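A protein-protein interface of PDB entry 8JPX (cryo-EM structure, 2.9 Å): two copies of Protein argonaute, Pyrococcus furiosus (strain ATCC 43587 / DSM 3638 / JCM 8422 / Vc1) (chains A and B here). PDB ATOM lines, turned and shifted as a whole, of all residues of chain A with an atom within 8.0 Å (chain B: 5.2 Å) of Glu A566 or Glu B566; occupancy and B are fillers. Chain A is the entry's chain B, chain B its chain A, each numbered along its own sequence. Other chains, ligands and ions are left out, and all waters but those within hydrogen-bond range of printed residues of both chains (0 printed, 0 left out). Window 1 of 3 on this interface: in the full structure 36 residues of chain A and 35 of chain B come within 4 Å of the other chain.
Of the 16 printed residues of chain A, 8 touch a printed residue of chain B. Of the 8 printed residues of chain B, 4 touch a printed residue of chain A. Among the printed residues, 13 pairs touch across the chains.
Of the printed residues of chain B, Lys A257 touches Arg B594 (3.3 Å). Printed residues of chain B within 4 Å of Ser A565: Ser B565, Glu B566 and Arg B594. Of the printed residues of chain B, Glu A592 touches Arg B564 and Ser B565. Lys B252 touches none of the printed residues of chain A. Printed residues of chain A within 4 Å of Ser B565: Ser A565 (3.2 Å), Glu A566 (3.5 Å), Glu A592 (3.7 Å) and Arg A594 (3.8 Å). Of the printed residues of chain A, Glu B566 touches Ser A565 and Glu A566. Of the printed residues of chain A, Arg B594 touches Lys A257 (3.3 Å), Lys A563 (3.8 Å), Arg A564 (3.3 Å) and Ser A565 (3.7 Å). The nearest residue of chain B that does not touch Glu A566 is Arg B594 (4.8 Å). The nearest residue of chain A that does not touch Glu B566 is Arg A594 (4.8 Å). The nearest printed residue of chain B that does not touch Lys A563 is Ser B565 (9.4 Å).
The side-chain carboxylate of Glu A566 lies within salt-bridge range of the side-chain amino group of Lys A255, 3.7 Å away. The side-chain sulfur (SD) of Met A562 lies within hydrogen-bond range of the side-chain hydroxyl (OG) of Ser A565 (3.5 Å). The backbone carbonyl oxygen (O) of Gln A593 lies within hydrogen-bond range of the backbone NH (N) of Tyr A568, at 2.9 Å. The backbone carbonyl oxygen of Gly A595 lies within hydrogen-bond range of the side-chain amide nitrogen of Gln A593, 2.9 Å away. OE2 of Glu B566 lies within salt-bridge range of NZ of Lys B255.
Arg B594 touches Lys A257 (CD to NZ, 3.3 Å). Arg B594 touches Lys A563 (NH2 to O, 3.8 Å). Arg B594 touches Arg A564. Glu B566 touches Ser A565 (O to OG, 3.7 Å). Ser A565 touches Arg B594. Ser B565 touches Glu A566. CG of Glu A592 touches O of Arg B564, 3.4 Å away. Gln A593 touches Arg B564. Arg B564 touches Arg A594. NH1 of Arg A594 touches N of Ser B565, 3.8 Å away.
OG of Ser A565 is in hydrogen-bond range of OG of Ser B565 (3.2 Å). The backbone NH of Glu A566 is in hydrogen-bond range of the backbone carbonyl oxygen of Glu B566, at 3.4 Å.
Arg A564 touches Arg B594, and with the chains exchanged Arg A594 touches Arg B564. Ser A565 touches its own counterpart, Ser B565. Ser A565 touches Arg B594, and with the chains exchanged Arg A594 touches Ser B565. Glu A566 touches its own counterpart, Glu B566. Of the 13 pairs that touch across the chains among the printed residues, 8 have their exchanged pair printed and touching as well.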
ATOM      1  N   SER A 251       5.858  25.802  -1.275  1.00  0.00           N
ATOM      2  CA  SER A 251       5.024  25.153  -2.270  1.00  0.00           C
ATOM      3  C   SER A 251       5.594  25.383  -3.668  1.00  0.00           C
ATOM      4  O   SER A 251       6.665  25.967  -3.844  1.00  0.00           O
ATOM      5  CB  SER A 251       3.588  25.664  -2.171  1.00  0.00           C
ATOM      6  OG  SER A 251       3.336  26.656  -3.150  1.00  0.00           O
ATOM      7  N   LYS A 252       4.865  24.909  -4.681  1.00  0.00           N
ATOM      8  CA  LYS A 252       5.299  25.070  -6.063  1.00  0.00           C
ATOM      9  C   LYS A 252       4.154  25.428  -7.004  1.00  0.00           C
ATOM     10  O   LYS A 252       4.362  25.444  -8.223  1.00  0.00           O
ATOM     11  CB  LYS A 252       5.992  23.797  -6.562  1.00  0.00           C
ATOM     12  CG  LYS A 252       7.455  23.696  -6.173  1.00  0.00           C
ATOM     13  CD  LYS A 252       7.776  22.325  -5.608  1.00  0.00           C
ATOM     14  CE  LYS A 252       7.453  22.252  -4.126  1.00  0.00           C
ATOM     15  NZ  LYS A 252       8.624  22.625  -3.285  1.00  0.00           N
ATOM     16  N   LYS A 255       4.990  28.401  -8.884  1.00  0.00           N
ATOM     17  CA  LYS A 255       6.078  28.066  -9.810  1.00  0.00           C
ATOM     18  C   LYS A 255       6.961  29.306  -9.969  1.00  0.00           C
ATOM     19  O   LYS A 255       7.064  30.123  -9.043  1.00  0.00           O
ATOM     20  CB  LYS A 255       5.511  27.512 -11.108  1.00  0.00           C
ATOM     21  CG  LYS A 255       6.397  26.476 -11.779  1.00  0.00           C
ATOM     22  CD  LYS A 255       6.764  25.358 -10.818  1.00  0.00           C
ATOM     23  CE  LYS A 255       7.935  24.545 -11.340  1.00  0.00           C
ATOM     24  NZ  LYS A 255       9.239  25.116 -10.909  1.00  0.00           N
ATOM     25  N   LYS A 257      10.390  29.569 -10.228  1.00  0.00           N
ATOM     26  CA  LYS A 257      11.315  29.421  -9.111  1.00  0.00           C
ATOM     27  C   LYS A 257      12.568  30.267  -9.304  1.00  0.00           C
ATOM     28  O   LYS A 257      13.695  29.780  -9.168  1.00  0.00           O
ATOM     29  CB  LYS A 257      11.678  27.948  -8.910  1.00  0.00           C
ATOM     30  CG  LYS A 257      12.188  27.237 -10.153  1.00  0.00           C
ATOM     31  CD  LYS A 257      12.371  25.755  -9.877  1.00  0.00           C
ATOM     32  CE  LYS A 257      13.673  25.494  -9.141  1.00  0.00           C
ATOM     33  NZ  LYS A 257      13.574  24.312  -8.245  1.00  0.00           N
ATOM     34  N   PRO A 561       7.711   9.744  -4.207  1.00  0.00           N
ATOM     35  CA  PRO A 561       8.263  10.906  -4.916  1.00  0.00           C
ATOM     36  C   PRO A 561       9.739  10.737  -5.234  1.00  0.00           C
ATOM     37  O   PRO A 561      10.393   9.836  -4.703  1.00  0.00           O
ATOM     38  CB  PRO A 561       8.032  12.065  -3.935  1.00  0.00           C
ATOM     39  CG  PRO A 561       7.112  11.535  -2.884  1.00  0.00           C
ATOM     40  CD  PRO A 561       7.357  10.070  -2.818  1.00  0.00           C
ATOM     41  N   MET A 562      10.274  11.597  -6.094  1.00  0.00           N
ATOM     42  CA  MET A 562      11.686  11.584  -6.445  1.00  0.00           C
ATOM     43  C   MET A 562      12.461  12.543  -5.548  1.00  0.00           C
ATOM     44  O   MET A 562      11.900  13.441  -4.919  1.00  0.00           O
ATOM     45  CB  MET A 562      11.880  11.958  -7.915  1.00  0.00           C
ATOM     46  CG  MET A 562      11.904  10.776  -8.860  1.00  0.00           C
ATOM     47  SD  MET A 562      11.972  11.285 -10.585  1.00  0.00           S
ATOM     48  CE  MET A 562      11.991   9.693 -11.396  1.00  0.00           C
ATOM     49  N   LYS A 563      13.779  12.343  -5.501  1.00  0.00           N
ATOM     50  CA  LYS A 563      14.614  13.152  -4.620  1.00  0.00           C
ATOM     51  C   LYS A 563      14.877  14.533  -5.213  1.00  0.00           C
ATOM     52  O   LYS A 563      14.502  15.552  -4.624  1.00  0.00           O
ATOM     53  CB  LYS A 563      15.929  12.428  -4.328  1.00  0.00           C
ATOM     54  CG  LYS A 563      16.764  13.098  -3.255  1.00  0.00           C
ATOM     55  CD  LYS A 563      16.577  12.424  -1.910  1.00  0.00           C
ATOM     56  CE  LYS A 563      17.078  10.995  -1.943  1.00  0.00           C
ATOM     57  NZ  LYS A 563      18.453  10.910  -2.504  1.00  0.00           N
ATOM     58  N   ARG A 564      15.522  14.589  -6.376  1.00  0.00           N
ATOM     59  CA  ARG A 564      15.765  15.852  -7.073  1.00  0.00           C
ATOM     60  C   ARG A 564      15.111  15.766  -8.446  1.00  0.00           C
ATOM     61  O   ARG A 564      15.775  15.498  -9.449  1.00  0.00           O
ATOM     62  CB  ARG A 564      17.260  16.138  -7.183  1.00  0.00           C
ATOM     63  CG  ARG A 564      18.032  15.931  -5.897  1.00  0.00           C
ATOM     64  CD  ARG A 564      19.526  15.887  -6.157  1.00  0.00           C
ATOM     65  NE  ARG A 564      20.173  14.783  -5.457  1.00  0.00           N
ATOM     66  CZ  ARG A 564      20.074  13.509  -5.808  1.00  0.00           C
ATOM     67  NH1 ARG A 564      19.368  13.134  -6.863  1.00  0.00           N
ATOM     68  NH2 ARG A 564      20.703  12.586  -5.086  1.00  0.00           N
ATOM     69  N   SER A 565      13.804  16.029  -8.482  1.00  0.00           N
ATOM     70  CA  SER A 565      13.013  16.063  -9.706  1.00  0.00           C
ATOM     71  C   SER A 565      11.565  16.372  -9.358  1.00  0.00           C
ATOM     72  O   SER A 565      11.209  16.448  -8.178  1.00  0.00           O
ATOM     73  CB  SER A 565      13.095  14.738 -10.466  1.00  0.00           C
ATOM     74  OG  SER A 565      12.056  14.640 -11.423  1.00  0.00           O
ATOM     75  N   GLU A 566      10.723  16.551 -10.370  1.00  0.00           N
ATOM     76  CA  GLU A 566       9.276  16.617 -10.184  1.00  0.00           C
ATOM     77  C   GLU A 566       8.693  15.407 -10.907  1.00  0.00           C
ATOM     78  O   GLU A 566       8.271  15.499 -12.062  1.00  0.00           O
ATOM     79  CB  GLU A 566       8.700  17.927 -10.703  1.00  0.00           C
ATOM     80  CG  GLU A 566       9.230  19.153  -9.983  1.00  0.00           C
ATOM     81  CD  GLU A 566       8.575  20.435 -10.455  1.00  0.00           C
ATOM     82  OE1 GLU A 566       7.667  20.362 -11.309  1.00  0.00           O
ATOM     83  OE2 GLU A 566       8.970  21.516  -9.971  1.00  0.00           O
ATOM     84  N   GLY A 567       8.667  14.277 -10.215  1.00  0.00           N
ATOM     85  CA  GLY A 567       8.201  13.036 -10.804  1.00  0.00           C
ATOM     86  C   GLY A 567       7.998  12.006  -9.719  1.00  0.00           C
ATOM     87  O   GLY A 567       8.204  12.271  -8.532  1.00  0.00           O
ATOM     88  N   TYR A 568       7.592  10.813 -10.142  1.00  0.00           N
ATOM     89  CA  TYR A 568       7.261   9.750  -9.205  1.00  0.00           C
ATOM     90  C   TYR A 568       7.833   8.430  -9.698  1.00  0.00           C
ATOM     91  O   TYR A 568       8.113   8.252 -10.884  1.00  0.00           O
ATOM     92  CB  TYR A 568       5.748   9.645  -8.999  1.00  0.00           C
ATOM     93  CG  TYR A 568       5.176  10.802  -8.216  1.00  0.00           C
ATOM     94  CD1 TYR A 568       4.803  11.976  -8.852  1.00  0.00           C
ATOM     95  CD2 TYR A 568       5.023  10.725  -6.842  1.00  0.00           C
ATOM     96  CE1 TYR A 568       4.290  13.037  -8.142  1.00  0.00           C
ATOM     97  CE2 TYR A 568       4.509  11.782  -6.124  1.00  0.00           C
ATOM     98  CZ  TYR A 568       4.145  12.934  -6.778  1.00  0.00           C
ATOM     99  OH  TYR A 568       3.632  13.989  -6.063  1.00  0.00           O
ATOM    100  N   GLU A 592       9.623   5.285 -14.148  1.00  0.00           N
ATOM    101  CA  GLU A 592       9.274   6.616 -13.684  1.00  0.00           C
ATOM    102  C   GLU A 592       7.976   7.091 -14.332  1.00  0.00           C
ATOM    103  O   GLU A 592       7.567   6.617 -15.396  1.00  0.00           O
ATOM    104  CB  GLU A 592      10.412   7.588 -13.985  1.00  0.00           C
ATOM    105  CG  GLU A 592      10.143   8.528 -15.142  1.00  0.00           C
ATOM    106  CD  GLU A 592      11.373   9.306 -15.547  1.00  0.00           C
ATOM    107  OE1 GLU A 592      11.655   9.386 -16.761  1.00  0.00           O
ATOM    108  OE2 GLU A 592      12.061   9.828 -14.649  1.00  0.00           O
ATOM    109  N   GLN A 593       7.321   8.044 -13.673  1.00  0.00           N
ATOM    110  CA  GLN A 593       6.028   8.529 -14.131  1.00  0.00           C
ATOM    111  C   GLN A 593       5.841   9.963 -13.665  1.00  0.00           C
ATOM    112  O   GLN A 593       6.611  10.476 -12.850  1.00  0.00           O
ATOM    113  CB  GLN A 593       4.892   7.642 -13.619  1.00  0.00           C
ATOM    114  CG  GLN A 593       4.830   7.559 -12.110  1.00  0.00           C
ATOM    115  CD  GLN A 593       4.151   6.303 -11.628  1.00  0.00           C
ATOM    116  OE1 GLN A 593       4.367   5.222 -12.170  1.00  0.00           O
ATOM    117  NE2 GLN A 593       3.327   6.435 -10.599  1.00  0.00           N
ATOM    118  N   ARG A 594       4.799  10.605 -14.194  1.00  0.00           N
ATOM    119  CA  ARG A 594       4.551  12.013 -13.912  1.00  0.00           C
ATOM    120  C   ARG A 594       3.621  12.236 -12.728  1.00  0.00           C
ATOM    121  O   ARG A 594       3.715  13.275 -12.066  1.00  0.00           O
ATOM    122  CB  ARG A 594       3.969  12.703 -15.147  1.00  0.00           C
ATOM    123  CG  ARG A 594       4.240  14.194 -15.193  1.00  0.00           C
ATOM    124  CD  ARG A 594       3.976  14.771 -16.572  1.00  0.00           C
ATOM    125  NE  ARG A 594       4.286  13.829 -17.639  1.00  0.00           N
ATOM    126  CZ  ARG A 594       5.197  14.036 -18.580  1.00  0.00           C
ATOM    127  NH1 ARG A 594       5.925  15.139 -18.605  1.00  0.00           N
ATOM    128  NH2 ARG A 594       5.379  13.115 -19.521  1.00  0.00           N
ATOM    129  N   GLY A 595       2.724  11.297 -12.445  1.00  0.00           N
ATOM    130  CA  GLY A 595       1.818  11.440 -11.324  1.00  0.00           C
ATOM    131  C   GLY A 595       1.664  10.162 -10.530  1.00  0.00           C
ATOM    132  O   GLY A 595       2.436   9.220 -10.716  1.00  0.00           O
ATOM    133  N   LYS B 252       4.372  24.820 -20.701  1.00  0.00           N
ATOM    134  CA  LYS B 252       4.067  24.470 -19.320  1.00  0.00           C
ATOM    135  C   LYS B 252       4.240  25.642 -18.360  1.00  0.00           C
ATOM    136  O   LYS B 252       4.157  25.439 -17.143  1.00  0.00           O
ATOM    137  CB  LYS B 252       4.938  23.297 -18.856  1.00  0.00           C
ATOM    138  CG  LYS B 252       4.408  21.934 -19.262  1.00  0.00           C
ATOM    139  CD  LYS B 252       5.510  21.077 -19.857  1.00  0.00           C
ATOM    140  CE  LYS B 252       5.689  21.364 -21.338  1.00  0.00           C
ATOM    141  NZ  LYS B 252       4.849  20.473 -22.183  1.00  0.00           N
ATOM    142  N   LYS B 255       1.248  26.104 -16.408  1.00  0.00           N
ATOM    143  CA  LYS B 255       1.122  24.960 -15.493  1.00  0.00           C
ATOM    144  C   LYS B 255      -0.369  24.677 -15.299  1.00  0.00           C
ATOM    145  O   LYS B 255      -1.178  24.941 -16.198  1.00  0.00           O
ATOM    146  CB  LYS B 255       1.897  25.224 -14.214  1.00  0.00           C
ATOM    147  CG  LYS B 255       2.471  23.972 -13.569  1.00  0.00           C
ATOM    148  CD  LYS B 255       3.292  23.169 -14.565  1.00  0.00           C
ATOM    149  CE  LYS B 255       3.524  21.751 -14.070  1.00  0.00           C
ATOM    150  NZ  LYS B 255       2.428  20.835 -14.489  1.00  0.00           N
ATOM    151  N   ARG B 564       9.294  10.907 -19.480  1.00  0.00           N
ATOM    152  CA  ARG B 564       8.034  11.258 -18.829  1.00  0.00           C
ATOM    153  C   ARG B 564       8.333  11.717 -17.404  1.00  0.00           C
ATOM    154  O   ARG B 564       8.203  10.959 -16.440  1.00  0.00           O
ATOM    155  CB  ARG B 564       7.046  10.067 -18.871  1.00  0.00           C
ATOM    156  CG  ARG B 564       7.607   8.746 -18.368  1.00  0.00           C
ATOM    157  CD  ARG B 564       6.689   7.588 -18.722  1.00  0.00           C
ATOM    158  NE  ARG B 564       6.983   7.015 -20.029  1.00  0.00           N
ATOM    159  CZ  ARG B 564       8.089   6.348 -20.329  1.00  0.00           C
ATOM    160  NH1 ARG B 564       9.033   6.129 -19.427  1.00  0.00           N
ATOM    161  NH2 ARG B 564       8.249   5.879 -21.563  1.00  0.00           N
ATOM    162  N   SER B 565       8.714  12.986 -17.279  1.00  0.00           N
ATOM    163  CA  SER B 565       8.983  13.653 -16.010  1.00  0.00           C
ATOM    164  C   SER B 565       9.387  15.083 -16.342  1.00  0.00           C
ATOM    165  O   SER B 565       9.541  15.447 -17.511  1.00  0.00           O
ATOM    166  CB  SER B 565      10.079  12.964 -15.196  1.00  0.00           C
ATOM    167  OG  SER B 565      10.548  13.812 -14.164  1.00  0.00           O
ATOM    168  N   GLU B 566       9.557  15.889 -15.301  1.00  0.00           N
ATOM    169  CA  GLU B 566      10.120  17.230 -15.431  1.00  0.00           C
ATOM    170  C   GLU B 566      11.465  17.214 -14.714  1.00  0.00           C
ATOM    171  O   GLU B 566      11.565  17.581 -13.542  1.00  0.00           O
ATOM    172  CB  GLU B 566       9.186  18.291 -14.866  1.00  0.00           C
ATOM    173  CG  GLU B 566       7.830  18.335 -15.544  1.00  0.00           C
ATOM    174  CD  GLU B 566       6.953  19.455 -15.021  1.00  0.00           C
ATOM    175  OE1 GLU B 566       7.418  20.220 -14.151  1.00  0.00           O
ATOM    176  OE2 GLU B 566       5.798  19.570 -15.481  1.00  0.00           O
ATOM    177  N   GLY B 567      12.499  16.795 -15.431  1.00  0.00           N
ATOM    178  CA  GLY B 567      13.824  16.679 -14.855  1.00  0.00           C
ATOM    179  C   GLY B 567      14.837  16.484 -15.958  1.00  0.00           C
ATOM    180  O   GLY B 567      14.502  16.472 -17.145  1.00  0.00           O
ATOM    181  N   TYR B 568      16.094  16.328 -15.551  1.00  0.00           N
ATOM    182  CA  TYR B 568      17.186  16.206 -16.502  1.00  0.00           C
ATOM    183  C   TYR B 568      18.152  15.127 -16.040  1.00  0.00           C
ATOM    184  O   TYR B 568      18.213  14.780 -14.859  1.00  0.00           O
ATOM    185  CB  TYR B 568      17.911  17.542 -16.688  1.00  0.00           C
ATOM    186  CG  TYR B 568      17.090  18.559 -17.440  1.00  0.00           C
ATOM    187  CD1 TYR B 568      16.189  19.378 -16.778  1.00  0.00           C
ATOM    188  CD2 TYR B 568      17.203  18.690 -18.815  1.00  0.00           C
ATOM    189  CE1 TYR B 568      15.431  20.302 -17.460  1.00  0.00           C
ATOM    190  CE2 TYR B 568      16.450  19.612 -19.506  1.00  0.00           C
ATOM    191  CZ  TYR B 568      15.565  20.414 -18.824  1.00  0.00           C
ATOM    192  OH  TYR B 568      14.812  21.333 -19.513  1.00  0.00           O
ATOM    193  N   ARG B 594      17.475  18.733 -11.436  1.00  0.00           N
ATOM    194  CA  ARG B 594      16.303  19.563 -11.685  1.00  0.00           C
ATOM    195  C   ARG B 594      16.479  20.517 -12.857  1.00  0.00           C
ATOM    196  O   ARG B 594      15.487  20.896 -13.488  1.00  0.00           O
ATOM    197  CB  ARG B 594      15.951  20.363 -10.428  1.00  0.00           C
ATOM    198  CG  ARG B 594      14.485  20.742 -10.339  1.00  0.00           C
ATOM    199  CD  ARG B 594      14.100  21.149  -8.928  1.00  0.00           C
ATOM    200  NE  ARG B 594      14.826  20.391  -7.916  1.00  0.00           N
ATOM    201  CZ  ARG B 594      14.254  19.605  -7.016  1.00  0.00           C
ATOM    202  NH1 ARG B 594      12.942  19.436  -6.979  1.00  0.00           N
ATOM    203  NH2 ARG B 594      15.016  18.975  -6.127  1.00  0.00           N
